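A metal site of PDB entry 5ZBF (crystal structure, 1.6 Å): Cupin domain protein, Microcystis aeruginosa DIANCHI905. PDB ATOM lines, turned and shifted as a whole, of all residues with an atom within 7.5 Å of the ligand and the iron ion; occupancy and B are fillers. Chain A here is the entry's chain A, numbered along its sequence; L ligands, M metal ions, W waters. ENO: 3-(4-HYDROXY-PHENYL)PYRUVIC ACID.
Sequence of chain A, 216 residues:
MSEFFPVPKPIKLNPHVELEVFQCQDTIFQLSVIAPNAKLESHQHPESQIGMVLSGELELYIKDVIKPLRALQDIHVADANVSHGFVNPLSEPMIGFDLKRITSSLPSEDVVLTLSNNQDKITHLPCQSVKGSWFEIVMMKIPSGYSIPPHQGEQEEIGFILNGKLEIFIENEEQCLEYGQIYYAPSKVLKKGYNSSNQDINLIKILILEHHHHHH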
ATOM      1  N   LEU A  13      -9.566   4.314  -6.089  1.00  0.00           N
ATOM      2  CA  LEU A  13     -10.741   3.963  -5.307  1.00  0.00           C
ATOM      3  C   LEU A  13     -10.556   2.599  -4.713  1.00  0.00           C
ATOM      4  O   LEU A  13     -10.988   2.322  -3.596  1.00  0.00           O
ATOM      5  CB  LEU A  13     -11.992   4.014  -6.174  1.00  0.00           C
ATOM      6  CG  LEU A  13     -13.296   4.384  -5.474  1.00  0.00           C
ATOM      7  CD1 LEU A  13     -13.143   5.649  -4.637  1.00  0.00           C
ATOM      8  CD2 LEU A  13     -14.405   4.543  -6.499  1.00  0.00           C
ATOM      9  N   ASN A  14      -9.925   1.731  -5.489  1.00  0.00           N
ATOM     10  CA  ASN A  14      -9.568   0.399  -5.038  1.00  0.00           C
ATOM     11  C   ASN A  14      -8.539  -0.047  -6.061  1.00  0.00           C
ATOM     12  O   ASN A  14      -8.165   0.752  -6.942  1.00  0.00           O
ATOM     13  CB  ASN A  14     -10.812  -0.507  -4.990  1.00  0.00           C
ATOM     14  CG  ASN A  14     -11.596  -0.508  -6.304  1.00  0.00           C
ATOM     15  OD1 ASN A  14     -11.109  -0.991  -7.322  1.00  0.00           O
ATOM     16  ND2 ASN A  14     -12.825   0.001  -6.269  1.00  0.00           N
ATOM     17  N   VAL A  17      -9.843   0.796  -9.758  1.00  0.00           N
ATOM     18  CA  VAL A  17     -10.441   2.033 -10.252  1.00  0.00           C
ATOM     19  C   VAL A  17      -9.601   3.254  -9.914  1.00  0.00           C
ATOM     20  O   VAL A  17      -9.312   3.532  -8.754  1.00  0.00           O
ATOM     21  CB  VAL A  17     -11.862   2.256  -9.671  1.00  0.00           C
ATOM     22  CG1 VAL A  17     -12.460   3.548 -10.205  1.00  0.00           C
ATOM     23  CG2 VAL A  17     -12.759   1.075 -10.001  1.00  0.00           C
ATOM     24  N   LEU A  19      -9.549   7.460 -10.615  1.00  0.00           N
ATOM     25  CA  LEU A  19     -10.436   8.559 -10.975  1.00  0.00           C
ATOM     26  C   LEU A  19      -9.691   9.896 -11.009  1.00  0.00           C
ATOM     27  O   LEU A  19      -8.731  10.099 -10.250  1.00  0.00           O
ATOM     28  CB  LEU A  19     -11.574   8.673  -9.976  1.00  0.00           C
ATOM     29  CG  LEU A  19     -12.499   7.477  -9.718  1.00  0.00           C
ATOM     30  CD1 LEU A  19     -13.488   7.819  -8.624  1.00  0.00           C
ATOM     31  CD2 LEU A  19     -13.245   7.052 -10.970  1.00  0.00           C
ATOM     32  N   GLN A  30     -16.342  12.929 -12.972  1.00  0.00           N
ATOM     33  CA  GLN A  30     -15.088  12.178 -12.905  1.00  0.00           C
ATOM     34  C   GLN A  30     -14.759  11.427 -14.173  1.00  0.00           C
ATOM     35  O   GLN A  30     -15.618  10.885 -14.829  1.00  0.00           O
ATOM     36  CB  GLN A  30     -15.091  11.222 -11.692  1.00  0.00           C
ATOM     37  CG  GLN A  30     -16.196  10.186 -11.712  1.00  0.00           C
ATOM     38  CD  GLN A  30     -16.410   9.515 -10.362  1.00  0.00           C
ATOM     39  OE1 GLN A  30     -16.219  10.112  -9.316  1.00  0.00           O
ATOM     40  NE2 GLN A  30     -16.841   8.263 -10.391  1.00  0.00           N
ATOM     41  N   SER A  32     -12.778   8.140 -15.366  1.00  0.00           N
ATOM     42  CA  SER A  32     -12.503   6.832 -14.759  1.00  0.00           C
ATOM     43  C   SER A  32     -11.590   5.982 -15.628  1.00  0.00           C
ATOM     44  O   SER A  32     -11.699   6.005 -16.845  1.00  0.00           O
ATOM     45  CB  SER A  32     -13.802   6.055 -14.577  1.00  0.00           C
ATOM     46  OG  SER A  32     -14.588   6.578 -13.524  1.00  0.00           O
ATOM     47  N   ILE A  34     -10.891   1.934 -15.390  1.00  0.00           N
ATOM     48  CA  ILE A  34     -11.180   0.651 -14.745  1.00  0.00           C
ATOM     49  C   ILE A  34     -10.274  -0.434 -15.336  1.00  0.00           C
ATOM     50  O   ILE A  34     -10.225  -0.639 -16.553  1.00  0.00           O
ATOM     51  CB  ILE A  34     -12.658   0.258 -14.878  1.00  0.00           C
ATOM     52  CG1 ILE A  34     -13.552   1.282 -14.168  1.00  0.00           C
ATOM     53  CG2 ILE A  34     -12.904  -1.148 -14.323  1.00  0.00           C
ATOM     54  CD1 ILE A  34     -15.031   0.985 -14.257  1.00  0.00           C
ATOM     55  N   LYS A  39     -13.894  -6.742 -11.605  1.00  0.00           N
ATOM     56  CA  LYS A  39     -15.211  -6.835 -10.994  1.00  0.00           C
ATOM     57  C   LYS A  39     -15.356  -5.734  -9.963  1.00  0.00           C
ATOM     58  O   LYS A  39     -14.541  -5.620  -9.057  1.00  0.00           O
ATOM     59  CB  LYS A  39     -15.404  -8.181 -10.288  1.00  0.00           C
ATOM     60  CG  LYS A  39     -15.520  -9.370 -11.214  1.00  0.00           C
ATOM     61  CD  LYS A  39     -15.451 -10.683 -10.474  1.00  0.00           C
ATOM     62  CE  LYS A  39     -16.547 -10.841  -9.446  1.00  0.00           C
ATOM     63  NZ  LYS A  39     -16.530 -12.214  -8.882  1.00  0.00           N
ATOM     64  N   LEU A  40     -16.409  -4.932 -10.111  1.00  0.00           N
ATOM     65  CA  LEU A  40     -16.702  -3.834  -9.186  1.00  0.00           C
ATOM     66  C   LEU A  40     -17.952  -4.198  -8.396  1.00  0.00           C
ATOM     67  O   LEU A  40     -19.034  -4.299  -8.964  1.00  0.00           O
ATOM     68  CB  LEU A  40     -16.961  -2.537  -9.952  1.00  0.00           C
ATOM     69  CG  LEU A  40     -15.819  -1.546 -10.180  1.00  0.00           C
ATOM     70  CD1 LEU A  40     -14.479  -2.231 -10.386  1.00  0.00           C
ATOM     71  CD2 LEU A  40     -16.134  -0.611 -11.337  1.00  0.00           C
ATOM     72  N   GLU A  41     -17.782  -4.400  -7.088  1.00  0.00           N
ATOM     73  CA  GLU A  41     -18.894  -4.746  -6.216  1.00  0.00           C
ATOM     74  C   GLU A  41     -19.960  -3.668  -6.254  1.00  0.00           C
ATOM     75  O   GLU A  41     -19.658  -2.476  -6.298  1.00  0.00           O
ATOM     76  CB  GLU A  41     -18.420  -4.943  -4.772  1.00  0.00           C
ATOM     77  CG  GLU A  41     -19.425  -5.664  -3.894  1.00  0.00           C
ATOM     78  N   SER A  42     -21.219  -4.093  -6.231  1.00  0.00           N
ATOM     79  CA  SER A  42     -22.333  -3.153  -6.236  1.00  0.00           C
ATOM     80  C   SER A  42     -22.264  -2.251  -5.012  1.00  0.00           C
ATOM     81  O   SER A  42     -21.890  -2.702  -3.916  1.00  0.00           O
ATOM     82  CB  SER A  42     -23.665  -3.903  -6.258  1.00  0.00           C
ATOM     83  OG  SER A  42     -23.761  -4.748  -7.389  1.00  0.00           O
ATOM     84  N   HIS A  43     -22.625  -0.995  -5.202  1.00  0.00           N
ATOM     85  CA  HIS A  43     -22.749  -0.063  -4.097  1.00  0.00           C
ATOM     86  C   HIS A  43     -23.961   0.809  -4.303  1.00  0.00           C
ATOM     87  O   HIS A  43     -24.617   0.746  -5.335  1.00  0.00           O
ATOM     88  CB  HIS A  43     -21.466   0.752  -3.883  1.00  0.00           C
ATOM     89  CG  HIS A  43     -21.177   1.769  -4.944  1.00  0.00           C
ATOM     90  ND1 HIS A  43     -20.004   2.495  -4.952  1.00  0.00           N
ATOM     91  CD2 HIS A  43     -21.892   2.179  -6.026  1.00  0.00           C
ATOM     92  CE1 HIS A  43     -20.004   3.320  -5.985  1.00  0.00           C
ATOM     93  NE2 HIS A  43     -21.146   3.154  -6.643  1.00  0.00           N
ATOM     94  N   GLN A  44     -24.289   1.601  -3.293  1.00  0.00           N
ATOM     95  CA  GLN A  44     -25.337   2.581  -3.408  1.00  0.00           C
ATOM     96  C   GLN A  44     -24.912   3.838  -2.701  1.00  0.00           C
ATOM     97  O   GLN A  44     -24.086   3.802  -1.779  1.00  0.00           O
ATOM     98  CB  GLN A  44     -26.672   2.035  -2.879  1.00  0.00           C
ATOM     99  CG  GLN A  44     -26.640   1.503  -1.462  1.00  0.00           C
ATOM    100  CD  GLN A  44     -27.776   0.529  -1.201  1.00  0.00           C
ATOM    101  OE1 GLN A  44     -27.537  -0.625  -0.869  1.00  0.00           O
ATOM    102  NE2 GLN A  44     -29.011   0.980  -1.358  1.00  0.00           N
ATOM    103  N   HIS A  45     -25.461   4.957  -3.149  1.00  0.00           N
ATOM    104  CA  HIS A  45     -25.198   6.248  -2.545  1.00  0.00           C
ATOM    105  C   HIS A  45     -26.344   7.188  -2.869  1.00  0.00           C
ATOM    106  O   HIS A  45     -27.047   6.987  -3.868  1.00  0.00           O
ATOM    107  CB  HIS A  45     -23.875   6.828  -3.062  1.00  0.00           C
ATOM    108  CG  HIS A  45     -23.608   6.540  -4.505  1.00  0.00           C
ATOM    109  ND1 HIS A  45     -24.336   7.132  -5.522  1.00  0.00           N
ATOM    110  CD2 HIS A  45     -22.694   5.753  -5.093  1.00  0.00           C
ATOM    111  CE1 HIS A  45     -23.870   6.710  -6.679  1.00  0.00           C
ATOM    112  NE2 HIS A  45     -22.875   5.867  -6.449  1.00  0.00           N
ATOM    113  N   GLU A  47     -26.362  10.154  -4.030  1.00  0.00           N
ATOM    114  CA  GLU A  47     -26.227  10.844  -5.316  1.00  0.00           C
ATOM    115  C   GLU A  47     -26.751   9.966  -6.433  1.00  0.00           C
ATOM    116  O   GLU A  47     -26.471   8.761  -6.488  1.00  0.00           O
ATOM    117  CB  GLU A  47     -24.780  11.222  -5.596  1.00  0.00           C
ATOM    118  CG  GLU A  47     -24.183  12.240  -4.630  1.00  0.00           C
ATOM    119  CD  GLU A  47     -23.655  11.634  -3.341  1.00  0.00           C
ATOM    120  OE1 GLU A  47     -23.614  10.384  -3.202  1.00  0.00           O
ATOM    121  OE2 GLU A  47     -23.271  12.418  -2.438  1.00  0.00           O
ATOM    122  N   SER A  48     -27.522  10.585  -7.331  1.00  0.00           N
ATOM    123  CA  SER A  48     -27.851   9.983  -8.610  1.00  0.00           C
ATOM    124  C   SER A  48     -26.623  10.007  -9.498  1.00  0.00           C
ATOM    125  O   SER A  48     -25.771  10.901  -9.360  1.00  0.00           O
ATOM    126  CB  SER A  48     -28.964  10.752  -9.305  1.00  0.00           C
ATOM    127  OG  SER A  48     -30.146  10.763  -8.523  1.00  0.00           O
ATOM    128  N   GLN A  49     -26.539   9.044 -10.411  1.00  0.00           N
ATOM    129  CA  GLN A  49     -25.343   8.851 -11.210  1.00  0.00           C
ATOM    130  C   GLN A  49     -25.688   8.490 -12.644  1.00  0.00           C
ATOM    131  O   GLN A  49     -26.602   7.699 -12.905  1.00  0.00           O
ATOM    132  CB  GLN A  49     -24.502   7.731 -10.577  1.00  0.00           C
ATOM    133  CG  GLN A  49     -23.222   7.387 -11.314  1.00  0.00           C
ATOM    134  CD  GLN A  49     -22.514   6.198 -10.685  1.00  0.00           C
ATOM    135  OE1 GLN A  49     -22.180   5.220 -11.357  1.00  0.00           O
ATOM    136  NE2 GLN A  49     -22.288   6.294  -9.390  1.00  0.00           N
ATOM    137  N   HIS A  76     -25.329   4.862 -18.764  1.00  0.00           N
ATOM    138  CA  HIS A  76     -25.940   4.162 -17.627  1.00  0.00           C
ATOM    139  C   HIS A  76     -26.594   5.199 -16.729  1.00  0.00           C
ATOM    140  O   HIS A  76     -26.102   6.325 -16.625  1.00  0.00           O
ATOM    141  CB  HIS A  76     -24.938   3.263 -16.871  1.00  0.00           C
ATOM    142  CG  HIS A  76     -23.999   3.997 -15.969  1.00  0.00           C
ATOM    143  ND1 HIS A  76     -22.714   4.329 -16.351  1.00  0.00           N
ATOM    144  CD2 HIS A  76     -24.133   4.448 -14.696  1.00  0.00           C
ATOM    145  CE1 HIS A  76     -22.113   4.963 -15.361  1.00  0.00           C
ATOM    146  NE2 HIS A  76     -22.953   5.051 -14.353  1.00  0.00           N
ATOM    147  N   ALA A  78     -28.214   5.453 -12.817  1.00  0.00           N
ATOM    148  CA  ALA A  78     -28.471   4.878 -11.491  1.00  0.00           C
ATOM    149  C   ALA A  78     -29.071   5.962 -10.609  1.00  0.00           C
ATOM    150  O   ALA A  78     -28.360   6.866 -10.145  1.00  0.00           O
ATOM    151  CB  ALA A  78     -27.189   4.349 -10.885  1.00  0.00           C
ATOM    152  N   VAL A  82     -29.985   3.458  -5.786  1.00  0.00           N
ATOM    153  CA  VAL A  82     -30.202   2.255  -6.586  1.00  0.00           C
ATOM    154  C   VAL A  82     -28.869   1.525  -6.620  1.00  0.00           C
ATOM    155  O   VAL A  82     -27.851   2.099  -7.004  1.00  0.00           O
ATOM    156  CB  VAL A  82     -30.674   2.582  -8.013  1.00  0.00           C
ATOM    157  CG1 VAL A  82     -30.718   1.343  -8.886  1.00  0.00           C
ATOM    158  CG2 VAL A  82     -32.031   3.257  -7.967  1.00  0.00           C
ATOM    159  N   HIS A  84     -25.848  -0.459  -7.769  1.00  0.00           N
ATOM    160  CA  HIS A  84     -25.238  -0.643  -9.093  1.00  0.00           C
ATOM    161  C   HIS A  84     -23.801  -1.112  -8.971  1.00  0.00           C
ATOM    162  O   HIS A  84     -23.060  -0.663  -8.083  1.00  0.00           O
ATOM    163  CB  HIS A  84     -25.313   0.638  -9.910  1.00  0.00           C
ATOM    164  CG  HIS A  84     -24.688   1.828  -9.255  1.00  0.00           C
ATOM    165  ND1 HIS A  84     -25.323   2.552  -8.271  1.00  0.00           N
ATOM    166  CD2 HIS A  84     -23.502   2.440  -9.471  1.00  0.00           C
ATOM    167  CE1 HIS A  84     -24.552   3.547  -7.896  1.00  0.00           C
ATOM    168  NE2 HIS A  84     -23.442   3.505  -8.610  1.00  0.00           N
ATOM    169  N   GLY A  85     -23.437  -2.016  -9.867  1.00  0.00           N
ATOM    170  CA  GLY A  85     -22.065  -2.539  -9.951  1.00  0.00           C
ATOM    171  C   GLY A  85     -21.684  -2.689 -11.402  1.00  0.00           C
ATOM    172  O   GLY A  85     -22.501  -2.464 -12.288  1.00  0.00           O
ATOM    173  N   PHE A  86     -20.433  -3.096 -11.641  1.00  0.00           N
ATOM    174  CA  PHE A  86     -19.904  -3.215 -12.994  1.00  0.00           C
ATOM    175  C   PHE A  86     -18.915  -4.369 -13.132  1.00  0.00           C
ATOM    176  O   PHE A  86     -18.240  -4.756 -12.169  1.00  0.00           O
ATOM    177  CB  PHE A  86     -19.158  -1.933 -13.404  1.00  0.00           C
ATOM    178  CG  PHE A  86     -20.008  -0.694 -13.351  1.00  0.00           C
ATOM    179  CD1 PHE A  86     -20.792  -0.321 -14.429  1.00  0.00           C
ATOM    180  CD2 PHE A  86     -19.993   0.134 -12.225  1.00  0.00           C
ATOM    181  CE1 PHE A  86     -21.570   0.828 -14.384  1.00  0.00           C
ATOM    182  CE2 PHE A  86     -20.753   1.294 -12.168  1.00  0.00           C
ATOM    183  CZ  PHE A  86     -21.546   1.641 -13.258  1.00  0.00           C
ATOM    184  N   ASP A  98     -18.282   9.643 -15.318  1.00  0.00           N
ATOM    185  CA  ASP A  98     -19.543   9.659 -14.565  1.00  0.00           C
ATOM    186  C   ASP A  98     -19.820  11.058 -14.065  1.00  0.00           C
ATOM    187  O   ASP A  98     -18.899  11.853 -13.865  1.00  0.00           O
ATOM    188  CB  ASP A  98     -19.487   8.768 -13.310  1.00  0.00           C
ATOM    189  CG  ASP A  98     -18.918   7.394 -13.560  1.00  0.00           C
ATOM    190  OD1 ASP A  98     -17.737   7.190 -13.199  1.00  0.00           O
ATOM    191  OD2 ASP A  98     -19.647   6.534 -14.077  1.00  0.00           O
ATOM    192  N   LYS A 100     -22.188  12.727 -10.815  1.00  0.00           N
ATOM    193  CA  LYS A 100     -22.961  12.422  -9.614  1.00  0.00           C
ATOM    194  C   LYS A 100     -23.489  13.700  -8.996  1.00  0.00           C
ATOM    195  O   LYS A 100     -22.785  14.713  -8.929  1.00  0.00           O
ATOM    196  CB  LYS A 100     -22.112  11.634  -8.613  1.00  0.00           C
ATOM    197  CG  LYS A 100     -21.825  10.208  -9.084  1.00  0.00           C
ATOM    198  CD  LYS A 100     -20.659   9.581  -8.336  1.00  0.00           C
ATOM    199  CE  LYS A 100     -20.987   9.362  -6.880  1.00  0.00           C
ATOM    200  NZ  LYS A 100     -19.946   8.482  -6.262  1.00  0.00           N
HETATM  201  O4  ENO L   1     -20.527   3.948  -9.499  1.00  0.00           O
HETATM  202  C9  ENO L   1     -16.813   2.130  -8.174  1.00  0.00           C
HETATM  203  C8  ENO L   1     -16.628   1.086  -7.279  1.00  0.00           C
HETATM  204  C7  ENO L   1     -17.641   0.141  -7.070  1.00  0.00           C
HETATM  205  C6  ENO L   1     -18.835   0.248  -7.778  1.00  0.00           C
HETATM  206  C5  ENO L   1     -19.014   1.296  -8.686  1.00  0.00           C
HETATM  207  C4  ENO L   1     -18.010   2.242  -8.890  1.00  0.00           C
HETATM  208  O3  ENO L   1     -17.459  -0.884  -6.187  1.00  0.00           O
HETATM  209  C3  ENO L   1     -18.243   3.378  -9.872  1.00  0.00           C
HETATM  210  C2  ENO L   1     -19.354   4.254  -9.306  1.00  0.00           C
HETATM  211  C1  ENO L   1     -19.025   5.438  -8.497  1.00  0.00           C
HETATM  212  O2  ENO L   1     -17.873   5.941  -8.533  1.00  0.00           O
HETATM  213  O1  ENO L   1     -19.935   5.923  -7.787  1.00  0.00           O
HETATM  214 FE    FE M   1     -21.795   4.750  -8.003  1.00  0.00          FE
HETATM  215  O   HOH W   1     -16.888   7.129  -6.104  1.00  0.00           O
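Leu 13 touches the ligand (CD2 to C9, 3.8 Å). CG of Leu 40 touches C7 of the ligand, at 3.98 Å. Phe 86 touches the ligand (CE2 to O4, 3.8 Å). Hydrophobic or aromatic side chains that line the ligand: Leu 13, Leu 40, His 43, His 45, His 84 and Phe 86. Ten residues have an atom within 4 Å of the ligand: Leu 13, Gln 30, Leu 40, Glu 41, His 43, His 45, Gln 49, His 84, Phe 86 and Lys 100.
Water W1 lies within hydrogen-bond range of an oxygen (O2) of the ligand (2.9 Å) and the side-chain amino group of Lys 100 (3.3 Å).
O3 of the ligand lies within hydrogen-bond range of O of Glu 41, 2.7 Å away. NZ of Lys 100 lies within salt-bridge range of O2 of the ligand, at 3.99 Å. The side-chain amide nitrogen of Gln 30 sits at hydrogen-bond distance from an oxygen (O2) of the ligand (3.1 Å).
The iron ion is bound by an oxygen (O4) of the ligand, 2.1 Å away. The iron ion is bound by NE2 of Gln 49 (2.1 Å). NE2 of His 84 is bound to the iron ion (2.2 Å). The iron ion is bound by NE2 of His 43 (2.2 Å). The iron ion is bound by a ring nitrogen (NE2) of His 45 (2.2 Å). An oxygen (O1) of the ligand is bound to the iron ion (2.2 Å). The iron ion has six donor atoms within binding distance.
ND1 of His 45 sits at hydrogen-bond distance from O of Glu 47 (2.9 Å). The backbone carbonyl oxygen of Gln 49 lies within hydrogen-bond range of the backbone NH of Ala 78. The backbone carbonyl oxygen (O) of Val 82 is in hydrogen-bond range of a ring nitrogen (ND1) of His 84, 2.9 Å away. OE1 of Gln 49 is in hydrogen-bond range of NE2 of His 76, 3.1 Å away. The backbone NH (N) of Gln 30 lies within hydrogen-bond range of the backbone carbonyl oxygen (O) of Asp 98 (2.9 Å). The backbone NH (N) of Leu 40 is in hydrogen-bond range of the backbone carbonyl oxygen (O) of Phe 86 (2.8 Å).
Of the 25 residues printed, 4 come within 4 Å of the iron ion.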
